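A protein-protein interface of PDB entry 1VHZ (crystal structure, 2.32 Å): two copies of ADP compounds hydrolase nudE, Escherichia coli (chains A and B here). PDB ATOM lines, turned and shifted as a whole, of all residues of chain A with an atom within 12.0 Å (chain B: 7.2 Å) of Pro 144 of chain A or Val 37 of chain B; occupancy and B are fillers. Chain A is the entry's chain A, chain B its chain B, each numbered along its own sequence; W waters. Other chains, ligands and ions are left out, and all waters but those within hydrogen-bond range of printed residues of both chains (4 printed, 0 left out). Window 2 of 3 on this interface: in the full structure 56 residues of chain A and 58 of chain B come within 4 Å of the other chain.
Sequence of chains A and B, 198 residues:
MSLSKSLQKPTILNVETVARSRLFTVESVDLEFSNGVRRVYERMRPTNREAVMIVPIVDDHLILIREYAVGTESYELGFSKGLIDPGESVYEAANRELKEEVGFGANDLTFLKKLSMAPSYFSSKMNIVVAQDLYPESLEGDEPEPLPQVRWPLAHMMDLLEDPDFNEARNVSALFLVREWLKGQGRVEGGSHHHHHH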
ATOM      1  N   ARG A  22     -20.531  13.304  20.053  1.00  0.00           N
ATOM      2  CA  ARG A  22     -21.346  14.384  20.608  1.00  0.00           C
ATOM      3  C   ARG A  22     -22.705  14.458  19.935  1.00  0.00           C
ATOM      4  O   ARG A  22     -23.703  14.776  20.585  1.00  0.00           O
ATOM      5  CB  ARG A  22     -20.606  15.720  20.537  1.00  0.00           C
ATOM      6  CG  ARG A  22     -21.138  16.779  21.494  1.00  0.00           C
ATOM      7  CD  ARG A  22     -20.115  17.898  21.696  1.00  0.00           C
ATOM      8  NE  ARG A  22     -19.701  18.455  20.410  1.00  0.00           N
ATOM      9  CZ  ARG A  22     -20.434  19.298  19.691  1.00  0.00           C
ATOM     10  NH1 ARG A  22     -21.622  19.697  20.125  1.00  0.00           N
ATOM     11  NH2 ARG A  22     -19.974  19.729  18.521  1.00  0.00           N
ATOM     12  N   ILE A  65     -31.680  28.816  -0.226  1.00  0.00           N
ATOM     13  CA  ILE A  65     -30.585  29.319   0.567  1.00  0.00           C
ATOM     14  C   ILE A  65     -29.294  28.544   0.258  1.00  0.00           C
ATOM     15  O   ILE A  65     -29.342  27.431  -0.247  1.00  0.00           O
ATOM     16  CB  ILE A  65     -30.827  29.272   2.085  1.00  0.00           C
ATOM     17  CG1 ILE A  65     -31.287  27.866   2.490  1.00  0.00           C
ATOM     18  CG2 ILE A  65     -31.852  30.313   2.523  1.00  0.00           C
ATOM     19  CD1 ILE A  65     -31.060  27.540   3.937  1.00  0.00           C
ATOM     20  N   ARG A  66     -28.151  29.171   0.525  1.00  0.00           N
ATOM     21  CA  ARG A  66     -26.844  28.558   0.343  1.00  0.00           C
ATOM     22  C   ARG A  66     -26.341  28.252   1.759  1.00  0.00           C
ATOM     23  O   ARG A  66     -26.419  29.108   2.635  1.00  0.00           O
ATOM     24  CB  ARG A  66     -25.896  29.426  -0.465  1.00  0.00           C
ATOM     25  CG  ARG A  66     -26.395  29.680  -1.886  1.00  0.00           C
ATOM     26  CD  ARG A  66     -25.430  30.542  -2.698  1.00  0.00           C
ATOM     27  NE  ARG A  66     -25.930  30.701  -4.063  1.00  0.00           N
ATOM     28  CZ  ARG A  66     -25.908  29.817  -5.044  1.00  0.00           C
ATOM     29  NH1 ARG A  66     -26.439  30.137  -6.233  1.00  0.00           N
ATOM     30  NH2 ARG A  66     -25.368  28.602  -4.885  1.00  0.00           N
ATOM     31  N   GLU A  67     -25.911  27.022   2.004  1.00  0.00           N
ATOM     32  CA  GLU A  67     -25.510  26.626   3.352  1.00  0.00           C
ATOM     33  C   GLU A  67     -24.359  25.645   3.331  1.00  0.00           C
ATOM     34  O   GLU A  67     -24.341  24.666   2.569  1.00  0.00           O
ATOM     35  CB  GLU A  67     -26.757  25.976   4.023  1.00  0.00           C
ATOM     36  CG  GLU A  67     -26.542  25.591   5.471  1.00  0.00           C
ATOM     37  CD  GLU A  67     -27.845  25.415   6.244  1.00  0.00           C
ATOM     38  OE1 GLU A  67     -27.859  25.631   7.475  1.00  0.00           O
ATOM     39  OE2 GLU A  67     -28.873  25.069   5.627  1.00  0.00           O
ATOM     40  N   TYR A  68     -23.376  25.902   4.203  1.00  0.00           N
ATOM     41  CA  TYR A  68     -22.215  25.036   4.242  1.00  0.00           C
ATOM     42  C   TYR A  68     -22.575  23.645   4.764  1.00  0.00           C
ATOM     43  O   TYR A  68     -23.365  23.493   5.683  1.00  0.00           O
ATOM     44  CB  TYR A  68     -21.084  25.661   5.052  1.00  0.00           C
ATOM     45  CG  TYR A  68     -19.821  24.835   5.100  1.00  0.00           C
ATOM     46  CD1 TYR A  68     -19.530  24.060   6.219  1.00  0.00           C
ATOM     47  CD2 TYR A  68     -18.933  24.801   4.033  1.00  0.00           C
ATOM     48  CE1 TYR A  68     -18.386  23.299   6.274  1.00  0.00           C
ATOM     49  CE2 TYR A  68     -17.771  24.056   4.086  1.00  0.00           C
ATOM     50  CZ  TYR A  68     -17.501  23.309   5.213  1.00  0.00           C
ATOM     51  OH  TYR A  68     -16.357  22.548   5.270  1.00  0.00           O
ATOM     52  N   ALA A  69     -21.963  22.645   4.162  1.00  0.00           N
ATOM     53  CA  ALA A  69     -22.144  21.238   4.523  1.00  0.00           C
ATOM     54  C   ALA A  69     -20.760  20.626   4.734  1.00  0.00           C
ATOM     55  O   ALA A  69     -19.975  20.497   3.783  1.00  0.00           O
ATOM     56  CB  ALA A  69     -22.877  20.535   3.372  1.00  0.00           C
ATOM     57  N   VAL A  70     -20.425  20.289   5.971  1.00  0.00           N
ATOM     58  CA  VAL A  70     -19.115  19.744   6.294  1.00  0.00           C
ATOM     59  C   VAL A  70     -18.867  18.361   5.739  1.00  0.00           C
ATOM     60  O   VAL A  70     -17.705  17.952   5.601  1.00  0.00           O
ATOM     61  CB  VAL A  70     -18.848  19.794   7.820  1.00  0.00           C
ATOM     62  CG1 VAL A  70     -19.540  18.661   8.551  1.00  0.00           C
ATOM     63  CG2 VAL A  70     -17.356  19.782   8.102  1.00  0.00           C
ATOM     64  N   SER A  74     -18.598  21.841   1.153  1.00  0.00           N
ATOM     65  CA  SER A  74     -19.029  22.710   0.060  1.00  0.00           C
ATOM     66  C   SER A  74     -20.326  23.395   0.483  1.00  0.00           C
ATOM     67  O   SER A  74     -20.899  23.054   1.517  1.00  0.00           O
ATOM     68  CB  SER A  74     -19.291  21.866  -1.204  1.00  0.00           C
ATOM     69  OG  SER A  74     -20.248  20.851  -0.889  1.00  0.00           O
ATOM     70  N   TYR A  75     -20.784  24.311  -0.351  1.00  0.00           N
ATOM     71  CA  TYR A  75     -22.012  25.025  -0.081  1.00  0.00           C
ATOM     72  C   TYR A  75     -23.145  24.363  -0.846  1.00  0.00           C
ATOM     73  O   TYR A  75     -23.007  24.124  -2.046  1.00  0.00           O
ATOM     74  CB  TYR A  75     -21.889  26.503  -0.459  1.00  0.00           C
ATOM     75  CG  TYR A  75     -21.202  27.286   0.641  1.00  0.00           C
ATOM     76  CD1 TYR A  75     -19.835  27.518   0.616  1.00  0.00           C
ATOM     77  CD2 TYR A  75     -21.947  27.753   1.726  1.00  0.00           C
ATOM     78  CE1 TYR A  75     -19.230  28.232   1.632  1.00  0.00           C
ATOM     79  CE2 TYR A  75     -21.344  28.447   2.743  1.00  0.00           C
ATOM     80  CZ  TYR A  75     -19.980  28.678   2.700  1.00  0.00           C
ATOM     81  OH  TYR A  75     -19.375  29.375   3.728  1.00  0.00           O
ATOM     82  N   LYS A  81     -34.041  24.043   6.102  1.00  0.00           N
ATOM     83  CA  LYS A  81     -34.350  22.853   6.864  1.00  0.00           C
ATOM     84  C   LYS A  81     -33.977  23.042   8.333  1.00  0.00           C
ATOM     85  O   LYS A  81     -32.985  23.719   8.629  1.00  0.00           O
ATOM     86  CB  LYS A  81     -33.447  21.679   6.355  1.00  0.00           C
ATOM     87  CG  LYS A  81     -33.719  21.246   4.942  1.00  0.00           C
ATOM     88  CD  LYS A  81     -32.698  20.336   4.307  1.00  0.00           C
ATOM     89  CE  LYS A  81     -32.888  20.232   2.795  1.00  0.00           C
ATOM     90  NZ  LYS A  81     -32.203  21.306   1.998  1.00  0.00           N
ATOM     91  N   GLU A  97     -38.514  28.322  11.842  1.00  0.00           N
ATOM     92  CA  GLU A  97     -37.314  28.135  11.040  1.00  0.00           C
ATOM     93  C   GLU A  97     -37.227  29.181   9.929  1.00  0.00           C
ATOM     94  O   GLU A  97     -36.119  29.670   9.686  1.00  0.00           O
ATOM     95  CB  GLU A  97     -37.205  26.737  10.431  1.00  0.00           C
ATOM     96  CG  GLU A  97     -36.997  25.608  11.427  1.00  0.00           C
ATOM     97  CD  GLU A  97     -35.593  25.586  12.013  1.00  0.00           C
ATOM     98  OE1 GLU A  97     -35.456  25.083  13.153  1.00  0.00           O
ATOM     99  OE2 GLU A  97     -34.643  26.055  11.344  1.00  0.00           O
ATOM    100  N   GLU A 100     -36.029  32.455  11.515  1.00  0.00           N
ATOM    101  CA  GLU A 100     -34.645  32.337  11.901  1.00  0.00           C
ATOM    102  C   GLU A 100     -33.692  32.316  10.706  1.00  0.00           C
ATOM    103  O   GLU A 100     -32.613  32.904  10.745  1.00  0.00           O
ATOM    104  CB  GLU A 100     -34.385  31.035  12.686  1.00  0.00           C
ATOM    105  CG  GLU A 100     -34.920  30.993  14.103  1.00  0.00           C
ATOM    106  CD  GLU A 100     -34.827  29.635  14.757  1.00  0.00           C
ATOM    107  OE1 GLU A 100     -35.474  29.444  15.809  1.00  0.00           O
ATOM    108  OE2 GLU A 100     -34.134  28.717  14.236  1.00  0.00           O
ATOM    109  N   GLU A 101     -34.077  31.646   9.616  1.00  0.00           N
ATOM    110  CA  GLU A 101     -33.124  31.537   8.510  1.00  0.00           C
ATOM    111  C   GLU A 101     -33.224  32.560   7.416  1.00  0.00           C
ATOM    112  O   GLU A 101     -32.206  32.979   6.855  1.00  0.00           O
ATOM    113  CB  GLU A 101     -33.250  30.118   7.911  1.00  0.00           C
ATOM    114  CG  GLU A 101     -32.879  29.049   8.946  1.00  0.00           C
ATOM    115  CD  GLU A 101     -32.680  27.681   8.327  1.00  0.00           C
ATOM    116  OE1 GLU A 101     -32.646  27.561   7.086  1.00  0.00           O
ATOM    117  OE2 GLU A 101     -32.547  26.704   9.094  1.00  0.00           O
ATOM    118  N   LEU A 139     -35.878  36.119  13.716  1.00  0.00           N
ATOM    119  CA  LEU A 139     -35.624  35.405  14.965  1.00  0.00           C
ATOM    120  C   LEU A 139     -34.148  34.963  14.932  1.00  0.00           C
ATOM    121  O   LEU A 139     -33.597  34.778  13.838  1.00  0.00           O
ATOM    122  CB  LEU A 139     -36.522  34.208  15.137  1.00  0.00           C
ATOM    123  CG  LEU A 139     -37.616  34.102  16.171  1.00  0.00           C
ATOM    124  CD1 LEU A 139     -38.180  35.423  16.667  1.00  0.00           C
ATOM    125  CD2 LEU A 139     -38.783  33.250  15.641  1.00  0.00           C
ATOM    126  N   GLU A 140     -33.544  34.818  16.088  1.00  0.00           N
ATOM    127  CA  GLU A 140     -32.160  34.413  16.232  1.00  0.00           C
ATOM    128  C   GLU A 140     -31.990  32.910  16.057  1.00  0.00           C
ATOM    129  O   GLU A 140     -32.518  32.119  16.829  1.00  0.00           O
ATOM    130  CB  GLU A 140     -31.625  34.805  17.619  1.00  0.00           C
ATOM    131  CG  GLU A 140     -30.540  35.861  17.615  1.00  0.00           C
ATOM    132  CD  GLU A 140     -29.139  35.283  17.540  1.00  0.00           C
ATOM    133  OE1 GLU A 140     -28.217  36.016  17.117  1.00  0.00           O
ATOM    134  OE2 GLU A 140     -28.935  34.100  17.902  1.00  0.00           O
ATOM    135  N   GLY A 141     -31.220  32.522  15.037  1.00  0.00           N
ATOM    136  CA  GLY A 141     -30.992  31.091  14.810  1.00  0.00           C
ATOM    137  C   GLY A 141     -29.614  30.715  15.347  1.00  0.00           C
ATOM    138  O   GLY A 141     -28.970  31.545  15.980  1.00  0.00           O
ATOM    139  N   ASP A 142     -29.160  29.499  15.063  1.00  0.00           N
ATOM    140  CA  ASP A 142     -27.856  29.061  15.537  1.00  0.00           C
ATOM    141  C   ASP A 142     -26.800  28.983  14.444  1.00  0.00           C
ATOM    142  O   ASP A 142     -25.718  28.428  14.702  1.00  0.00           O
ATOM    143  CB  ASP A 142     -27.952  27.678  16.218  1.00  0.00           C
ATOM    144  CG  ASP A 142     -29.007  27.681  17.309  1.00  0.00           C
ATOM    145  OD1 ASP A 142     -28.814  28.412  18.302  1.00  0.00           O
ATOM    146  OD2 ASP A 142     -30.030  26.978  17.150  1.00  0.00           O
ATOM    147  N   GLU A 143     -27.094  29.476  13.253  1.00  0.00           N
ATOM    148  CA  GLU A 143     -26.127  29.448  12.166  1.00  0.00           C
ATOM    149  C   GLU A 143     -24.905  30.308  12.482  1.00  0.00           C
ATOM    150  O   GLU A 143     -24.990  31.418  12.992  1.00  0.00           O
ATOM    151  CB  GLU A 143     -26.750  29.874  10.842  1.00  0.00           C
ATOM    152  CG  GLU A 143     -27.232  31.287  10.701  1.00  0.00           C
ATOM    153  CD  GLU A 143     -28.394  31.664  11.603  1.00  0.00           C
ATOM    154  OE1 GLU A 143     -28.479  32.849  11.980  1.00  0.00           O
ATOM    155  OE2 GLU A 143     -29.234  30.799  11.937  1.00  0.00           O
ATOM    156  N   PRO A 144     -23.727  29.792  12.129  1.00  0.00           N
ATOM    157  CA  PRO A 144     -22.476  30.489  12.351  1.00  0.00           C
ATOM    158  C   PRO A 144     -22.283  31.620  11.359  1.00  0.00           C
ATOM    159  O   PRO A 144     -21.494  32.524  11.590  1.00  0.00           O
ATOM    160  CB  PRO A 144     -21.417  29.419  12.179  1.00  0.00           C
ATOM    161  CG  PRO A 144     -22.031  28.367  11.330  1.00  0.00           C
ATOM    162  CD  PRO A 144     -23.523  28.452  11.531  1.00  0.00           C
ATOM    163  N   GLU A 145     -22.944  31.526  10.199  1.00  0.00           N
ATOM    164  CA  GLU A 145     -22.788  32.593   9.203  1.00  0.00           C
ATOM    165  C   GLU A 145     -24.120  32.784   8.502  1.00  0.00           C
ATOM    166  O   GLU A 145     -24.955  31.881   8.536  1.00  0.00           O
ATOM    167  CB  GLU A 145     -21.650  32.290   8.228  1.00  0.00           C
ATOM    168  CG  GLU A 145     -21.848  31.101   7.334  1.00  0.00           C
ATOM    169  CD  GLU A 145     -20.743  30.722   6.386  1.00  0.00           C
ATOM    170  OE1 GLU A 145     -19.721  31.417   6.179  1.00  0.00           O
ATOM    171  OE2 GLU A 145     -20.886  29.625   5.782  1.00  0.00           O
ATOM    172  N   PRO A 146     -24.346  33.957   7.945  1.00  0.00           N
ATOM    173  CA  PRO A 146     -25.575  34.248   7.236  1.00  0.00           C
ATOM    174  C   PRO A 146     -25.806  33.281   6.080  1.00  0.00           C
ATOM    175  O   PRO A 146     -24.866  32.712   5.512  1.00  0.00           O
ATOM    176  CB  PRO A 146     -25.410  35.682   6.750  1.00  0.00           C
ATOM    177  CG  PRO A 146     -24.256  36.250   7.494  1.00  0.00           C
ATOM    178  CD  PRO A 146     -23.392  35.092   7.907  1.00  0.00           C
ATOM    179  N   LEU A 147     -27.062  33.005   5.773  1.00  0.00           N
ATOM    180  CA  LEU A 147     -27.436  32.113   4.680  1.00  0.00           C
ATOM    181  C   LEU A 147     -27.887  32.926   3.476  1.00  0.00           C
ATOM    182  O   LEU A 147     -28.974  33.511   3.488  1.00  0.00           O
ATOM    183  CB  LEU A 147     -28.568  31.194   5.173  1.00  0.00           C
ATOM    184  CG  LEU A 147     -28.231  30.442   6.467  1.00  0.00           C
ATOM    185  CD1 LEU A 147     -29.464  29.829   7.109  1.00  0.00           C
ATOM    186  CD2 LEU A 147     -27.168  29.379   6.198  1.00  0.00           C
ATOM    187  N   PRO A 148     -27.049  33.043   2.465  1.00  0.00           N
ATOM    188  CA  PRO A 148     -27.395  33.823   1.281  1.00  0.00           C
ATOM    189  C   PRO A 148     -28.654  33.241   0.650  1.00  0.00           C
ATOM    190  O   PRO A 148     -28.803  32.019   0.610  1.00  0.00           O
ATOM    191  CB  PRO A 148     -26.186  33.725   0.368  1.00  0.00           C
ATOM    192  CG  PRO A 148     -25.074  33.235   1.215  1.00  0.00           C
ATOM    193  CD  PRO A 148     -25.714  32.439   2.344  1.00  0.00           C
ATOM    194  N   PRO B  10     -15.321  27.919   4.998  1.00  0.00           N
ATOM    195  CA  PRO B  10     -14.650  27.982   6.287  1.00  0.00           C
ATOM    196  C   PRO B  10     -13.341  27.204   6.168  1.00  0.00           C
ATOM    197  O   PRO B  10     -13.238  26.285   5.330  1.00  0.00           O
ATOM    198  CB  PRO B  10     -15.606  27.259   7.222  1.00  0.00           C
ATOM    199  CG  PRO B  10     -16.414  26.371   6.325  1.00  0.00           C
ATOM    200  CD  PRO B  10     -16.612  27.193   5.070  1.00  0.00           C
ATOM    201  N   LEU B  13      -9.552  23.642  10.577  1.00  0.00           N
ATOM    202  CA  LEU B  13      -8.395  23.734  11.450  1.00  0.00           C
ATOM    203  C   LEU B  13      -7.926  22.386  11.960  1.00  0.00           C
ATOM    204  O   LEU B  13      -6.728  22.172  12.164  1.00  0.00           O
ATOM    205  CB  LEU B  13      -8.734  24.637  12.652  1.00  0.00           C
ATOM    206  CG  LEU B  13      -9.309  26.011  12.251  1.00  0.00           C
ATOM    207  CD1 LEU B  13      -9.858  26.723  13.469  1.00  0.00           C
ATOM    208  CD2 LEU B  13      -8.255  26.839  11.543  1.00  0.00           C
ATOM    209  N   LEU B  31     -13.869  24.145  12.652  1.00  0.00           N
ATOM    210  CA  LEU B  31     -14.005  25.086  11.563  1.00  0.00           C
ATOM    211  C   LEU B  31     -13.884  26.537  12.003  1.00  0.00           C
ATOM    212  O   LEU B  31     -14.233  26.900  13.116  1.00  0.00           O
ATOM    213  CB  LEU B  31     -15.423  24.960  10.930  1.00  0.00           C
ATOM    214  CG  LEU B  31     -15.697  23.585  10.294  1.00  0.00           C
ATOM    215  CD1 LEU B  31     -17.181  23.352  10.089  1.00  0.00           C
ATOM    216  CD2 LEU B  31     -14.946  23.458   8.972  1.00  0.00           C
ATOM    217  N   GLU B  32     -13.388  27.327  11.050  1.00  0.00           N
ATOM    218  CA  GLU B  32     -13.287  28.757  11.211  1.00  0.00           C
ATOM    219  C   GLU B  32     -13.966  29.357   9.955  1.00  0.00           C
ATOM    220  O   GLU B  32     -13.435  29.202   8.859  1.00  0.00           O
ATOM    221  CB  GLU B  32     -11.897  29.323  11.363  1.00  0.00           C
ATOM    222  CG  GLU B  32     -11.918  30.852  11.456  1.00  0.00           C
ATOM    223  CD  GLU B  32     -10.544  31.451  11.695  1.00  0.00           C
ATOM    224  OE1 GLU B  32     -10.496  32.648  12.049  1.00  0.00           O
ATOM    225  OE2 GLU B  32      -9.536  30.746  11.513  1.00  0.00           O
ATOM    226  N   PHE B  33     -15.144  29.929  10.172  1.00  0.00           N
ATOM    227  CA  PHE B  33     -15.876  30.525   9.049  1.00  0.00           C
ATOM    228  C   PHE B  33     -15.189  31.794   8.608  1.00  0.00           C
ATOM    229  O   PHE B  33     -14.363  32.329   9.361  1.00  0.00           O
ATOM    230  CB  PHE B  33     -17.361  30.724   9.433  1.00  0.00           C
ATOM    231  CG  PHE B  33     -18.024  29.366   9.577  1.00  0.00           C
ATOM    232  CD1 PHE B  33     -17.914  28.653  10.768  1.00  0.00           C
ATOM    233  CD2 PHE B  33     -18.709  28.807   8.523  1.00  0.00           C
ATOM    234  CE1 PHE B  33     -18.476  27.386  10.893  1.00  0.00           C
ATOM    235  CE2 PHE B  33     -19.277  27.543   8.643  1.00  0.00           C
ATOM    236  CZ  PHE B  33     -19.155  26.837   9.830  1.00  0.00           C
ATOM    237  N   SER B  34     -15.520  32.337   7.444  1.00  0.00           N
ATOM    238  CA  SER B  34     -14.875  33.542   6.957  1.00  0.00           C
ATOM    239  C   SER B  34     -15.153  34.762   7.818  1.00  0.00           C
ATOM    240  O   SER B  34     -14.377  35.714   7.759  1.00  0.00           O
ATOM    241  CB  SER B  34     -15.238  33.796   5.495  1.00  0.00           C
ATOM    242  OG  SER B  34     -16.573  34.253   5.400  1.00  0.00           O
ATOM    243  N   ASN B  35     -16.183  34.766   8.654  1.00  0.00           N
ATOM    244  CA  ASN B  35     -16.502  35.880   9.534  1.00  0.00           C
ATOM    245  C   ASN B  35     -15.813  35.739  10.881  1.00  0.00           C
ATOM    246  O   ASN B  35     -16.164  36.420  11.848  1.00  0.00           O
ATOM    247  CB  ASN B  35     -18.025  35.976   9.738  1.00  0.00           C
ATOM    248  CG  ASN B  35     -18.617  34.730  10.376  1.00  0.00           C
ATOM    249  OD1 ASN B  35     -17.888  33.810  10.751  1.00  0.00           O
ATOM    250  ND2 ASN B  35     -19.940  34.698  10.549  1.00  0.00           N
ATOM    251  N   GLY B  36     -14.915  34.762  11.024  1.00  0.00           N
ATOM    252  CA  GLY B  36     -14.212  34.540  12.276  1.00  0.00           C
ATOM    253  C   GLY B  36     -14.892  33.587  13.239  1.00  0.00           C
ATOM    254  O   GLY B  36     -14.248  33.139  14.199  1.00  0.00           O
ATOM    255  N   VAL B  37     -16.167  33.248  13.054  1.00  0.00           N
ATOM    256  CA  VAL B  37     -16.843  32.324  13.978  1.00  0.00           C
ATOM    257  C   VAL B  37     -16.247  30.930  13.957  1.00  0.00           C
ATOM    258  O   VAL B  37     -15.943  30.380  12.889  1.00  0.00           O
ATOM    259  CB  VAL B  37     -18.337  32.252  13.610  1.00  0.00           C
ATOM    260  CG1 VAL B  37     -19.066  31.210  14.430  1.00  0.00           C
ATOM    261  CG2 VAL B  37     -18.955  33.639  13.775  1.00  0.00           C
ATOM    262  N   ARG B  38     -16.064  30.309  15.120  1.00  0.00           N
ATOM    263  CA  ARG B  38     -15.482  28.986  15.207  1.00  0.00           C
ATOM    264  C   ARG B  38     -16.501  27.975  15.703  1.00  0.00           C
ATOM    265  O   ARG B  38     -17.301  28.315  16.560  1.00  0.00           O
ATOM    266  CB  ARG B  38     -14.238  28.927  16.105  1.00  0.00           C
ATOM    267  CG  ARG B  38     -13.164  29.894  15.633  1.00  0.00           C
ATOM    268  CD  ARG B  38     -11.765  29.408  15.924  1.00  0.00           C
ATOM    269  NE  ARG B  38     -10.775  30.399  15.455  1.00  0.00           N
ATOM    270  CZ  ARG B  38      -9.473  30.219  15.647  1.00  0.00           C
ATOM    271  NH1 ARG B  38      -8.612  31.129  15.214  1.00  0.00           N
ATOM    272  NH2 ARG B  38      -9.068  29.126  16.282  1.00  0.00           N
ATOM    273  N   ARG B  39     -16.523  26.798  15.086  1.00  0.00           N
ATOM    274  CA  ARG B  39     -17.438  25.743  15.455  1.00  0.00           C
ATOM    275  C   ARG B  39     -16.772  24.365  15.299  1.00  0.00           C
ATOM    276  O   ARG B  39     -15.822  24.170  14.540  1.00  0.00           O
ATOM    277  CB  ARG B  39     -18.701  25.684  14.590  1.00  0.00           C
ATOM    278  CG  ARG B  39     -19.691  26.799  14.713  1.00  0.00           C
ATOM    279  CD  ARG B  39     -20.333  26.914  16.101  1.00  0.00           C
ATOM    280  NE  ARG B  39     -21.190  28.107  16.123  1.00  0.00           N
ATOM    281  CZ  ARG B  39     -22.426  28.129  15.626  1.00  0.00           C
ATOM    282  NH1 ARG B  39     -22.961  27.042  15.084  1.00  0.00           N
ATOM    283  NH2 ARG B  39     -23.119  29.249  15.658  1.00  0.00           N
ATOM    284  N   TYR B  41     -17.933  20.816  14.173  1.00  0.00           N
ATOM    285  CA  TYR B  41     -19.000  20.020  13.572  1.00  0.00           C
ATOM    286  C   TYR B  41     -18.618  18.538  13.639  1.00  0.00           C
ATOM    287  O   TYR B  41     -17.455  18.186  13.764  1.00  0.00           O
ATOM    288  CB  TYR B  41     -19.246  20.384  12.119  1.00  0.00           C
ATOM    289  CG  TYR B  41     -20.078  21.593  11.801  1.00  0.00           C
ATOM    290  CD1 TYR B  41     -20.317  22.587  12.730  1.00  0.00           C
ATOM    291  CD2 TYR B  41     -20.595  21.772  10.515  1.00  0.00           C
ATOM    292  CE1 TYR B  41     -21.087  23.697  12.433  1.00  0.00           C
ATOM    293  CE2 TYR B  41     -21.338  22.891  10.192  1.00  0.00           C
ATOM    294  CZ  TYR B  41     -21.577  23.852  11.158  1.00  0.00           C
ATOM    295  OH  TYR B  41     -22.332  24.960  10.858  1.00  0.00           O
HETATM  296  O   HOH W   1     -14.517  23.921   4.219  1.00  0.00           O
HETATM  297  O   HOH W   2     -23.347  25.056   8.407  1.00  0.00           O
HETATM  298  O   HOH W   3     -18.810  33.755   7.159  1.00  0.00           O
HETATM  299  O   HOH W   4     -17.061  30.704   5.816  1.00  0.00           O
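O of Pro 144 of chain A sits at hydrogen-bond distance from ND2 of Asn 35 of chain B (2.9 Å). NH2 of Arg 39 of chain B lies within hydrogen-bond range of O of Asp 142 of chain A (2.9 Å).
The backbone carbonyl oxygen (O) of Arg 39 of chain B is in hydrogen-bond range of the backbone NH (N) of Leu 31 of chain B. The side-chain carboxylate (OE2) of Glu 145 of chain A sits at hydrogen-bond distance from the side-chain hydroxyl (OH) of Tyr 75 of chain A (2.6 Å). The backbone NH (N) of Val 37 of chain B lies within hydrogen-bond range of the side-chain amide oxygen (OD1) of Asn 35 of chain B (2.9 Å).
Among the printed residues, pairs that only touch across the chains: Tyr 68 of chain A with Pro 10 of chain B (3.4 Å), Pro 144 of chain A with Tyr 41 of chain B (3.5 Å), Glu 145 of chain A with Phe 33 of chain B (3.5 Å), Pro 144 of chain A with Val 37 of chain B (3.5 Å), Pro 144 of chain A with Phe 33 of chain B (3.6 Å), Pro 144 of chain A with Arg 39 of chain B (3.6 Å), Glu 145 of chain A with Asn 35 of chain B (3.8 Å), Tyr 75 of chain A with Pro 10 of chain B (3.8 Å), Val 70 of chain A with Tyr 41 of chain B (3.8 Å) and Glu 143 of chain A with Arg 39 of chain B (3.8 Å).
Of chain B, only Phe 33, Asn 35, Val 37, Arg 39 and Tyr 41 come within 4 Å of Pro 144 of chain A. Of chain A, only Pro 144 comes within 4 Å of Val 37 of chain B. Phe 33 of chain B touches two residues of chain A. No residue of chain A comes within 4 Å of Ser 34 of chain B. No residue of chain A comes within 4 Å of Gly 36 of chain B. Arg 38 of chain B touches none of the printed residues of chain A. Of the printed residues of chain B, Tyr 75 of chain A touches Pro 10. Printed residues of chain B within 4 Å of Val 70 of chain A: Tyr 41 (3.8 Å). Of the printed residues of chain B, Asp 142 of chain A touches Arg 39 (2.9 Å). Printed residues of chain A within 4 Å of Tyr 41 of chain B: Val 70 (3.8 Å) and Pro 144 (3.5 Å). Lys 81 of chain A touches none of the printed residues of chain B. The nearest residue of chain B that does not touch Pro 144 of chain A is Arg 38 of chain B (6.1 Å). The nearest residue of chain A that does not touch Val 37 of chain B is Glu 145 of chain A (5.7 Å). The nearest printed residue of chain A that does not touch Tyr 41 of chain B is Tyr 68 of chain A (4.5 Å).
Of the 12 printed residues of chain B, 6 touch a printed residue of chain A. Hydrophobic or aromatic side chains of chain B within 4 Å of the printed part of chain A: Pro 10, Phe 33, Val 37 and Tyr 41. Among the printed residues, 12 pairs touch across the chains.
No position is printed for both chains. Of the 12 pairs that touch across the chains among the printed residues, none has its exchanged pair printed and touching as well.
Water W1 bridges the side-chain hydroxyl of Tyr 68 of chain A and the backbone carbonyl oxygen of Pro 10 of chain B. Water W2 lies within hydrogen-bond range of OH of Tyr 41 of chain B (2.7 Å) and O of Tyr 68 of chain A (3.1 Å). Water W3 lies within hydrogen-bond range of OE1 of Glu 145 of chain A, OG of Ser 34 of chain B and N of Asn 35 of chain B. Water W4 lies within hydrogen-bond range of N of Ser 34 of chain B (2.8 Å), OE1 of Glu 145 of chain A (2.8 Å) and OH of Tyr 75 of chain A (3.4 Å).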
